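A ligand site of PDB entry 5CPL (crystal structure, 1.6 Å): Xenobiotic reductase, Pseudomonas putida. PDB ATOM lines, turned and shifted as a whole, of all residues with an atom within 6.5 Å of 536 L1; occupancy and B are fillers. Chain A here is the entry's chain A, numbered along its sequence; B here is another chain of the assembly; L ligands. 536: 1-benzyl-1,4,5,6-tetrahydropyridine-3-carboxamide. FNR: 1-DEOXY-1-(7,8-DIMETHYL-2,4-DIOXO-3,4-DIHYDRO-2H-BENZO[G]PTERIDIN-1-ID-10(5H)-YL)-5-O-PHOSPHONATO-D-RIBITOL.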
ATOM      1  N   PRO A  23      -8.984  20.580  -1.083  1.00  0.00           N
ATOM      2  CA  PRO A  23      -9.475  21.946  -1.149  1.00  0.00           C
ATOM      3  C   PRO A  23     -10.962  22.009  -0.815  1.00  0.00           C
ATOM      4  O   PRO A  23     -11.741  21.179  -1.294  1.00  0.00           O
ATOM      5  CB  PRO A  23      -9.200  22.341  -2.617  1.00  0.00           C
ATOM      6  CG  PRO A  23      -9.153  21.007  -3.379  1.00  0.00           C
ATOM      7  CD  PRO A  23      -8.473  20.089  -2.374  1.00  0.00           C
ATOM      8  N   CYS A  25     -13.734  25.137  -0.596  1.00  0.00           N
ATOM      9  CA  CYS A  25     -14.234  26.523  -0.627  1.00  0.00           C
ATOM     10  C   CYS A  25     -14.953  26.899   0.657  1.00  0.00           C
ATOM     11  O   CYS A  25     -15.802  26.142   1.150  1.00  0.00           O
ATOM     12  CB  CYS A  25     -15.202  26.696  -1.792  1.00  0.00           C
ATOM     13  SG  CYS A  25     -14.377  26.768  -3.411  1.00  0.00           S
ATOM     14  N   TYR A  27     -16.193  30.284   0.902  1.00  0.00           N
ATOM     15  CA  TYR A  27     -17.099  31.342   0.447  1.00  0.00           C
ATOM     16  C   TYR A  27     -17.114  32.543   1.396  1.00  0.00           C
ATOM     17  O   TYR A  27     -18.132  33.216   1.532  1.00  0.00           O
ATOM     18  CB  TYR A  27     -18.515  30.798   0.266  1.00  0.00           C
ATOM     19  CG  TYR A  27     -18.584  29.513  -0.532  1.00  0.00           C
ATOM     20  CD1 TYR A  27     -18.684  29.538  -1.921  1.00  0.00           C
ATOM     21  CD2 TYR A  27     -18.504  28.274   0.088  1.00  0.00           C
ATOM     22  CE1 TYR A  27     -18.709  28.374  -2.663  1.00  0.00           C
ATOM     23  CE2 TYR A  27     -18.550  27.108  -0.661  1.00  0.00           C
ATOM     24  CZ  TYR A  27     -18.663  27.165  -2.021  1.00  0.00           C
ATOM     25  OH  TYR A  27     -18.697  26.027  -2.774  1.00  0.00           O
ATOM     26  N   ALA A  57     -10.139  26.016  -3.786  1.00  0.00           N
ATOM     27  CA  ALA A  57     -10.149  26.595  -5.128  1.00  0.00           C
ATOM     28  C   ALA A  57      -9.980  28.104  -5.075  1.00  0.00           C
ATOM     29  O   ALA A  57     -10.862  28.809  -4.587  1.00  0.00           O
ATOM     30  CB  ALA A  57     -11.444  26.228  -5.843  1.00  0.00           C
ATOM     31  N   ILE A  66     -16.108  30.921  -8.310  1.00  0.00           N
ATOM     32  CA  ILE A  66     -17.459  30.359  -8.395  1.00  0.00           C
ATOM     33  C   ILE A  66     -18.472  31.409  -7.942  1.00  0.00           C
ATOM     34  O   ILE A  66     -19.503  31.598  -8.580  1.00  0.00           O
ATOM     35  CB  ILE A  66     -17.593  29.089  -7.533  1.00  0.00           C
ATOM     36  CG1 ILE A  66     -16.522  28.075  -7.931  1.00  0.00           C
ATOM     37  CG2 ILE A  66     -18.982  28.486  -7.719  1.00  0.00           C
ATOM     38  CD1 ILE A  66     -16.390  26.908  -6.949  1.00  0.00           C
ATOM     39  N   GLN A  99      -4.948  24.884  -4.481  1.00  0.00           N
ATOM     40  CA  GLN A  99      -5.609  24.569  -5.723  1.00  0.00           C
ATOM     41  C   GLN A  99      -5.917  25.877  -6.449  1.00  0.00           C
ATOM     42  O   GLN A  99      -6.675  26.707  -5.922  1.00  0.00           O
ATOM     43  CB  GLN A  99      -6.895  23.784  -5.448  1.00  0.00           C
ATOM     44  CG  GLN A  99      -7.592  23.344  -6.742  1.00  0.00           C
ATOM     45  CD  GLN A  99      -8.984  22.807  -6.483  1.00  0.00           C
ATOM     46  OE1 GLN A  99      -9.865  23.514  -5.974  1.00  0.00           O
ATOM     47  NE2 GLN A  99      -9.191  21.563  -6.823  1.00  0.00           N
ATOM     48  N   PRO A 112     -23.428  28.523  -1.386  1.00  0.00           N
ATOM     49  CA  PRO A 112     -24.303  27.346  -1.347  1.00  0.00           C
ATOM     50  C   PRO A 112     -25.501  27.496  -0.400  1.00  0.00           C
ATOM     51  O   PRO A 112     -26.553  26.933  -0.687  1.00  0.00           O
ATOM     52  CB  PRO A 112     -23.349  26.232  -0.890  1.00  0.00           C
ATOM     53  CG  PRO A 112     -22.014  26.667  -1.426  1.00  0.00           C
ATOM     54  CD  PRO A 112     -22.007  28.170  -1.242  1.00  0.00           C
ATOM     55  N   HIS A 178      -6.925  22.899 -10.911  1.00  0.00           N
ATOM     56  CA  HIS A 178      -8.292  22.427 -10.820  1.00  0.00           C
ATOM     57  C   HIS A 178      -8.894  22.153 -12.198  1.00  0.00           C
ATOM     58  O   HIS A 178      -9.510  23.031 -12.812  1.00  0.00           O
ATOM     59  CB  HIS A 178      -9.169  23.441 -10.095  1.00  0.00           C
ATOM     60  CG  HIS A 178     -10.440  22.839  -9.582  1.00  0.00           C
ATOM     61  ND1 HIS A 178     -10.876  21.585  -9.969  1.00  0.00           N
ATOM     62  CD2 HIS A 178     -11.353  23.304  -8.697  1.00  0.00           C
ATOM     63  CE1 HIS A 178     -12.002  21.302  -9.326  1.00  0.00           C
ATOM     64  NE2 HIS A 178     -12.314  22.337  -8.556  1.00  0.00           N
ATOM     65  N   ALA A 180     -11.103  19.700 -12.590  1.00  0.00           N
ATOM     66  CA  ALA A 180     -12.248  18.844 -12.274  1.00  0.00           C
ATOM     67  C   ALA A 180     -13.560  19.600 -12.050  1.00  0.00           C
ATOM     68  O   ALA A 180     -13.634  20.807 -12.179  1.00  0.00           O
ATOM     69  CB  ALA A 180     -11.918  17.986 -11.061  1.00  0.00           C
ATOM     70  N   HIS A 181     -14.626  18.844 -11.791  1.00  0.00           N
ATOM     71  CA  HIS A 181     -15.893  19.348 -11.237  1.00  0.00           C
ATOM     72  C   HIS A 181     -16.618  20.310 -12.162  1.00  0.00           C
ATOM     73  O   HIS A 181     -17.440  21.126 -11.709  1.00  0.00           O
ATOM     74  CB  HIS A 181     -15.644  19.975  -9.866  1.00  0.00           C
ATOM     75  CG  HIS A 181     -15.070  19.002  -8.882  1.00  0.00           C
ATOM     76  ND1 HIS A 181     -14.529  19.391  -7.674  1.00  0.00           N
ATOM     77  CD2 HIS A 181     -14.909  17.670  -8.959  1.00  0.00           C
ATOM     78  CE1 HIS A 181     -14.070  18.323  -7.036  1.00  0.00           C
ATOM     79  NE2 HIS A 181     -14.304  17.265  -7.799  1.00  0.00           N
ATOM     80  N   TYR A 183     -15.731  22.798 -14.031  1.00  0.00           N
ATOM     81  CA  TYR A 183     -15.200  24.137 -14.225  1.00  0.00           C
ATOM     82  C   TYR A 183     -14.391  24.206 -15.527  1.00  0.00           C
ATOM     83  O   TYR A 183     -14.505  23.334 -16.383  1.00  0.00           O
ATOM     84  CB  TYR A 183     -14.402  24.533 -12.980  1.00  0.00           C
ATOM     85  CG  TYR A 183     -15.233  24.412 -11.724  1.00  0.00           C
ATOM     86  CD1 TYR A 183     -16.433  25.128 -11.568  1.00  0.00           C
ATOM     87  CD2 TYR A 183     -14.842  23.590 -10.678  1.00  0.00           C
ATOM     88  CE1 TYR A 183     -17.211  24.990 -10.410  1.00  0.00           C
ATOM     89  CE2 TYR A 183     -15.607  23.458  -9.517  1.00  0.00           C
ATOM     90  CZ  TYR A 183     -16.777  24.156  -9.389  1.00  0.00           C
ATOM     91  OH  TYR A 183     -17.531  24.005  -8.241  1.00  0.00           O
ATOM     92  N   ARG A 231      -6.248  18.103 -10.185  1.00  0.00           N
ATOM     93  CA  ARG A 231      -7.476  17.368  -9.915  1.00  0.00           C
ATOM     94  C   ARG A 231      -8.241  17.236 -11.231  1.00  0.00           C
ATOM     95  O   ARG A 231      -8.330  18.192 -11.987  1.00  0.00           O
ATOM     96  CB  ARG A 231      -8.323  18.064  -8.834  1.00  0.00           C
ATOM     97  CG  ARG A 231      -9.399  17.157  -8.265  1.00  0.00           C
ATOM     98  CD  ARG A 231     -10.019  17.711  -6.967  1.00  0.00           C
ATOM     99  NE  ARG A 231     -10.435  16.607  -6.095  1.00  0.00           N
ATOM    100  CZ  ARG A 231     -11.046  16.781  -4.929  1.00  0.00           C
ATOM    101  NH1 ARG A 231     -11.420  17.982  -4.523  1.00  0.00           N
ATOM    102  NH2 ARG A 231     -11.315  15.725  -4.173  1.00  0.00           N
ATOM    103  N   PHE A 269     -18.729  16.181 -12.901  1.00  0.00           N
ATOM    104  CA  PHE A 269     -19.798  17.155 -12.611  1.00  0.00           C
ATOM    105  C   PHE A 269     -19.965  18.135 -13.769  1.00  0.00           C
ATOM    106  O   PHE A 269     -20.314  19.286 -13.550  1.00  0.00           O
ATOM    107  CB  PHE A 269     -19.551  17.941 -11.302  1.00  0.00           C
ATOM    108  CG  PHE A 269     -19.300  17.085 -10.096  1.00  0.00           C
ATOM    109  CD1 PHE A 269     -19.949  15.865  -9.927  1.00  0.00           C
ATOM    110  CD2 PHE A 269     -18.398  17.481  -9.135  1.00  0.00           C
ATOM    111  CE1 PHE A 269     -19.704  15.087  -8.815  1.00  0.00           C
ATOM    112  CE2 PHE A 269     -18.153  16.703  -8.022  1.00  0.00           C
ATOM    113  CZ  PHE A 269     -18.798  15.502  -7.869  1.00  0.00           C
ATOM    114  N   TRP A 278     -23.126   7.733  -5.130  1.00  0.00           N
ATOM    115  CA  TRP A 278     -22.512   8.159  -3.895  1.00  0.00           C
ATOM    116  C   TRP A 278     -22.551   7.046  -2.859  1.00  0.00           C
ATOM    117  O   TRP A 278     -23.593   6.405  -2.651  1.00  0.00           O
ATOM    118  CB  TRP A 278     -23.224   9.375  -3.318  1.00  0.00           C
ATOM    119  CG  TRP A 278     -23.368  10.522  -4.243  1.00  0.00           C
ATOM    120  CD1 TRP A 278     -24.502  10.913  -4.893  1.00  0.00           C
ATOM    121  CD2 TRP A 278     -22.348  11.452  -4.607  1.00  0.00           C
ATOM    122  NE1 TRP A 278     -24.247  12.033  -5.641  1.00  0.00           N
ATOM    123  CE2 TRP A 278     -22.931  12.388  -5.482  1.00  0.00           C
ATOM    124  CE3 TRP A 278     -20.996  11.590  -4.288  1.00  0.00           C
ATOM    125  CZ2 TRP A 278     -22.219  13.445  -6.031  1.00  0.00           C
ATOM    126  CZ3 TRP A 278     -20.291  12.641  -4.827  1.00  0.00           C
ATOM    127  CH2 TRP A 278     -20.902  13.548  -5.692  1.00  0.00           C
ATOM    128  N   TRP A 302     -14.280  11.564  -0.939  1.00  0.00           N
ATOM    129  CA  TRP A 302     -15.684  11.244  -0.842  1.00  0.00           C
ATOM    130  C   TRP A 302     -16.148   9.939   0.110  1.00  0.00           C
ATOM    131  O   TRP A 302     -16.084   8.704  -0.222  1.00  0.00           O
ATOM    132  CB  TRP A 302     -16.216  11.167  -2.324  1.00  0.00           C
ATOM    133  CG  TRP A 302     -15.771  12.354  -3.379  1.00  0.00           C
ATOM    134  CD1 TRP A 302     -14.739  12.314  -4.332  1.00  0.00           C
ATOM    135  CD2 TRP A 302     -16.398  13.652  -3.585  1.00  0.00           C
ATOM    136  NE1 TRP A 302     -14.702  13.484  -5.053  1.00  0.00           N
ATOM    137  CE2 TRP A 302     -15.705  14.326  -4.620  1.00  0.00           C
ATOM    138  CE3 TRP A 302     -17.485  14.313  -2.981  1.00  0.00           C
ATOM    139  CZ2 TRP A 302     -16.052  15.615  -5.065  1.00  0.00           C
ATOM    140  CZ3 TRP A 302     -17.821  15.596  -3.430  1.00  0.00           C
ATOM    141  CH2 TRP A 302     -17.103  16.227  -4.455  1.00  0.00           C
ATOM    142  N   ARG A 326     -15.012  16.804   4.628  1.00  0.00           N
ATOM    143  CA  ARG A 326     -16.059  17.213   5.548  1.00  0.00           C
ATOM    144  C   ARG A 326     -15.802  16.802   7.004  1.00  0.00           C
ATOM    145  O   ARG A 326     -16.159  17.533   7.909  1.00  0.00           O
ATOM    146  CB  ARG A 326     -17.407  16.696   5.083  1.00  0.00           C
ATOM    147  CG  ARG A 326     -17.994  17.567   3.971  1.00  0.00           C
ATOM    148  CD  ARG A 326     -19.148  16.917   3.220  1.00  0.00           C
ATOM    149  NE  ARG A 326     -18.696  15.756   2.496  1.00  0.00           N
ATOM    150  CZ  ARG A 326     -19.483  15.001   1.735  1.00  0.00           C
ATOM    151  NH1 ARG A 326     -20.776  15.320   1.615  1.00  0.00           N
ATOM    152  NH2 ARG A 326     -18.993  13.936   1.106  1.00  0.00           N
ATOM    153  N   TRP B 358     -22.757  22.155   4.944  1.00  0.00           N
ATOM    154  CA  TRP B 358     -22.308  20.906   4.370  1.00  0.00           C
ATOM    155  C   TRP B 358     -22.492  19.734   5.293  1.00  0.00           C
ATOM    156  O   TRP B 358     -22.459  18.587   4.856  1.00  0.00           O
ATOM    157  CB  TRP B 358     -20.845  21.013   3.983  1.00  0.00           C
ATOM    158  CG  TRP B 358     -20.617  22.113   3.009  1.00  0.00           C
ATOM    159  CD1 TRP B 358     -20.213  23.411   3.282  1.00  0.00           C
ATOM    160  CD2 TRP B 358     -20.819  22.038   1.604  1.00  0.00           C
ATOM    161  NE1 TRP B 358     -20.145  24.113   2.119  1.00  0.00           N
ATOM    162  CE2 TRP B 358     -20.494  23.301   1.070  1.00  0.00           C
ATOM    163  CE3 TRP B 358     -21.204  21.023   0.727  1.00  0.00           C
ATOM    164  CZ2 TRP B 358     -20.554  23.578  -0.295  1.00  0.00           C
ATOM    165  CZ3 TRP B 358     -21.275  21.306  -0.632  1.00  0.00           C
ATOM    166  CH2 TRP B 358     -20.948  22.562  -1.130  1.00  0.00           C
HETATM  167  C1  536 L   1     -18.603  19.540  -5.471  1.00  0.00           C
HETATM  168  N2  536 L   1     -18.169  20.891  -5.194  1.00  0.00           N
HETATM  169  C3  536 L   1     -16.843  21.229  -5.502  1.00  0.00           C
HETATM  170  C4  536 L   1     -16.464  22.509  -5.434  1.00  0.00           C
HETATM  171  C5  536 L   1     -17.175  23.599  -4.650  1.00  0.00           C
HETATM  172  C6  536 L   1     -18.339  22.984  -3.883  1.00  0.00           C
HETATM  173  C7  536 L   1     -19.043  21.906  -4.690  1.00  0.00           C
HETATM  174  C8  536 L   1     -15.173  22.875  -6.131  1.00  0.00           C
HETATM  175  O9  536 L   1     -14.528  22.066  -6.795  1.00  0.00           O
HETATM  176  N10 536 L   1     -14.715  24.192  -5.856  1.00  0.00           N
HETATM  177  C11 536 L   1     -19.277  18.873  -4.253  1.00  0.00           C
HETATM  178  C12 536 L   1     -20.375  18.100  -4.445  1.00  0.00           C
HETATM  179  C13 536 L   1     -21.055  17.442  -3.255  1.00  0.00           C
HETATM  180  C14 536 L   1     -20.564  17.617  -1.996  1.00  0.00           C
HETATM  181  C15 536 L   1     -19.336  18.464  -1.791  1.00  0.00           C
HETATM  182  C16 536 L   1     -18.732  19.066  -2.848  1.00  0.00           C
HETATM  183  C9A FNR L   2     -15.617  20.872  -1.619  1.00  0.00           C
HETATM  184  N10 FNR L   2     -14.817  20.187  -2.621  1.00  0.00           N
HETATM  185  CAA FNR L   2     -13.909  20.955  -3.463  1.00  0.00           C
HETATM  186  N1  FNR L   2     -13.260  20.346  -4.432  1.00  0.00           N
HETATM  187  C2  FNR L   2     -12.301  20.981  -5.103  1.00  0.00           C
HETATM  188  O2  FNR L   2     -11.713  20.403  -5.971  1.00  0.00           O
HETATM  189  N3  FNR L   2     -12.032  22.283  -4.770  1.00  0.00           N
HETATM  190  C4  FNR L   2     -12.716  22.937  -3.839  1.00  0.00           C
HETATM  191  O4  FNR L   2     -12.434  24.076  -3.517  1.00  0.00           O
HETATM  192  C4A FNR L   2     -13.837  22.296  -3.348  1.00  0.00           C
HETATM  193  N5  FNR L   2     -14.707  22.962  -2.389  1.00  0.00           N
HETATM  194  C5A FNR L   2     -15.573  22.237  -1.500  1.00  0.00           C
HETATM  195  C6  FNR L   2     -16.057  22.880  -0.381  1.00  0.00           C
HETATM  196  C7  FNR L   2     -16.717  22.135   0.578  1.00  0.00           C
HETATM  197  C7M FNR L   2     -17.195  22.890   1.798  1.00  0.00           C
HETATM  198  C8  FNR L   2     -16.869  20.778   0.395  1.00  0.00           C
HETATM  199  C8M FNR L   2     -17.590  19.951   1.436  1.00  0.00           C
HETATM  200  C9  FNR L   2     -16.383  20.158  -0.709  1.00  0.00           C
HETATM  201  C1' FNR L   2     -14.821  18.734  -2.675  1.00  0.00           C
HETATM  202  C2' FNR L   2     -13.880  18.196  -1.583  1.00  0.00           C
HETATM  203  O2' FNR L   2     -12.543  18.516  -1.904  1.00  0.00           O
HETATM  204  C3' FNR L   2     -13.989  16.682  -1.401  1.00  0.00           C
HETATM  205  O3' FNR L   2     -13.692  16.004  -2.600  1.00  0.00           O
HETATM  206  C4' FNR L   2     -15.381  16.277  -0.918  1.00  0.00           C
HETATM  207  O4' FNR L   2     -15.738  17.031   0.224  1.00  0.00           O
HETATM  208  C5' FNR L   2     -15.468  14.780  -0.622  1.00  0.00           C
HETATM  209  O5' FNR L   2     -14.629  14.385   0.432  1.00  0.00           O
HETATM  210  P   FNR L   2     -15.303  14.142   1.895  1.00  0.00           P
HETATM  211  O1P FNR L   2     -15.938  15.448   2.339  1.00  0.00           O
HETATM  212  O2P FNR L   2     -14.147  13.750   2.764  1.00  0.00           O
HETATM  213  O3P FNR L   2     -16.358  13.042   1.810  1.00  0.00           O
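ND1 of His 181 lies within hydrogen-bond range of O9 of 536 L1, at 2.8 Å.
A ring nitrogen (NE2) of His 178 sits at hydrogen-bond distance from an oxygen (O9) of 536 L1, 2.8 Å away.
SG of Cys 25 lies within hydrogen-bond range of N10 of 536 L1.
An oxygen (O2) of FNR L2 lies close to a ring nitrogen (ND1) of His 181 (3.4 Å).
NE2 of His 178 is in hydrogen-bond range of O2 of FNR L2, 3.3 Å away.
The backbone NH of Trp 302 lies within hydrogen-bond range of an oxygen (O5') of FNR L2, at 3.2 Å.
An oxygen (O4) of FNR L2 lies close to the backbone NH (N) of Cys 25 (3.4 Å).
An oxygen (O4) of FNR L2 sits at hydrogen-bond distance from the side-chain sulfur (SG) of Cys 25, 3.3 Å away.
O4 of FNR L2 lies within hydrogen-bond range of N of Ala 57 (3.0 Å).
An oxygen (O1P) of FNR L2 lies within hydrogen-bond range of the backbone NH (N) of Arg 326, 2.8 Å away.
O1P of FNR L2 is in salt-bridge range of NE of Arg 326 (2.8 Å).
OE1 of Gln 99 sits at hydrogen-bond distance from N3 of FNR L2.
NH1 of Arg 231 sits at hydrogen-bond distance from O2 of FNR L2, at 2.8 Å.
An oxygen (O2') of FNR L2 lies within hydrogen-bond range of the backbone carbonyl oxygen (O) of Pro 23 (2.8 Å).
O9 of 536 L1 sits close to N1 of FNR L2, at 3.2 Å.
A ring nitrogen (ND1) of His 178 sits at hydrogen-bond distance from the backbone NH (N) of Ala 180 (3.2 Å).
The side-chain amide oxygen of Gln 99 lies close to the backbone NH of Ala 57, at 3.3 Å.
OH of Tyr 27 touches C6 of 536 L1, at 3.3 Å.
Ala 57 touches 536 L1 (CB to N10, 3.9 Å).
Ile 66 touches 536 L1.
CE2 of Tyr 183 touches O9 of 536 L1, 3.2 Å away.
CE2 of Phe 269 touches C1 of 536 L1, at 3.8 Å.
CH2 of Trp 302 touches C11 of 536 L1, 3.4 Å away.
Trp 358 of chain B touches 536 L1 (CZ3 to C15, 3.6 Å).
Hydrophobic or aromatic side chains that line 536 L1: Ala 57, Ile 66, His 178, His 181, Tyr 183, Phe 269, Trp 302 and Trp 358 of chain B.
Ten residues have an atom within 4 Å of 536 L1: Cys 25, Tyr 27, Ala 57, Ile 66, His 178, His 181, Tyr 183, Phe 269, Trp 302 and Trp 358 of chain B.
The nearest printed residue that does not touch 536 L1 is Arg 326 (4.3 Å).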
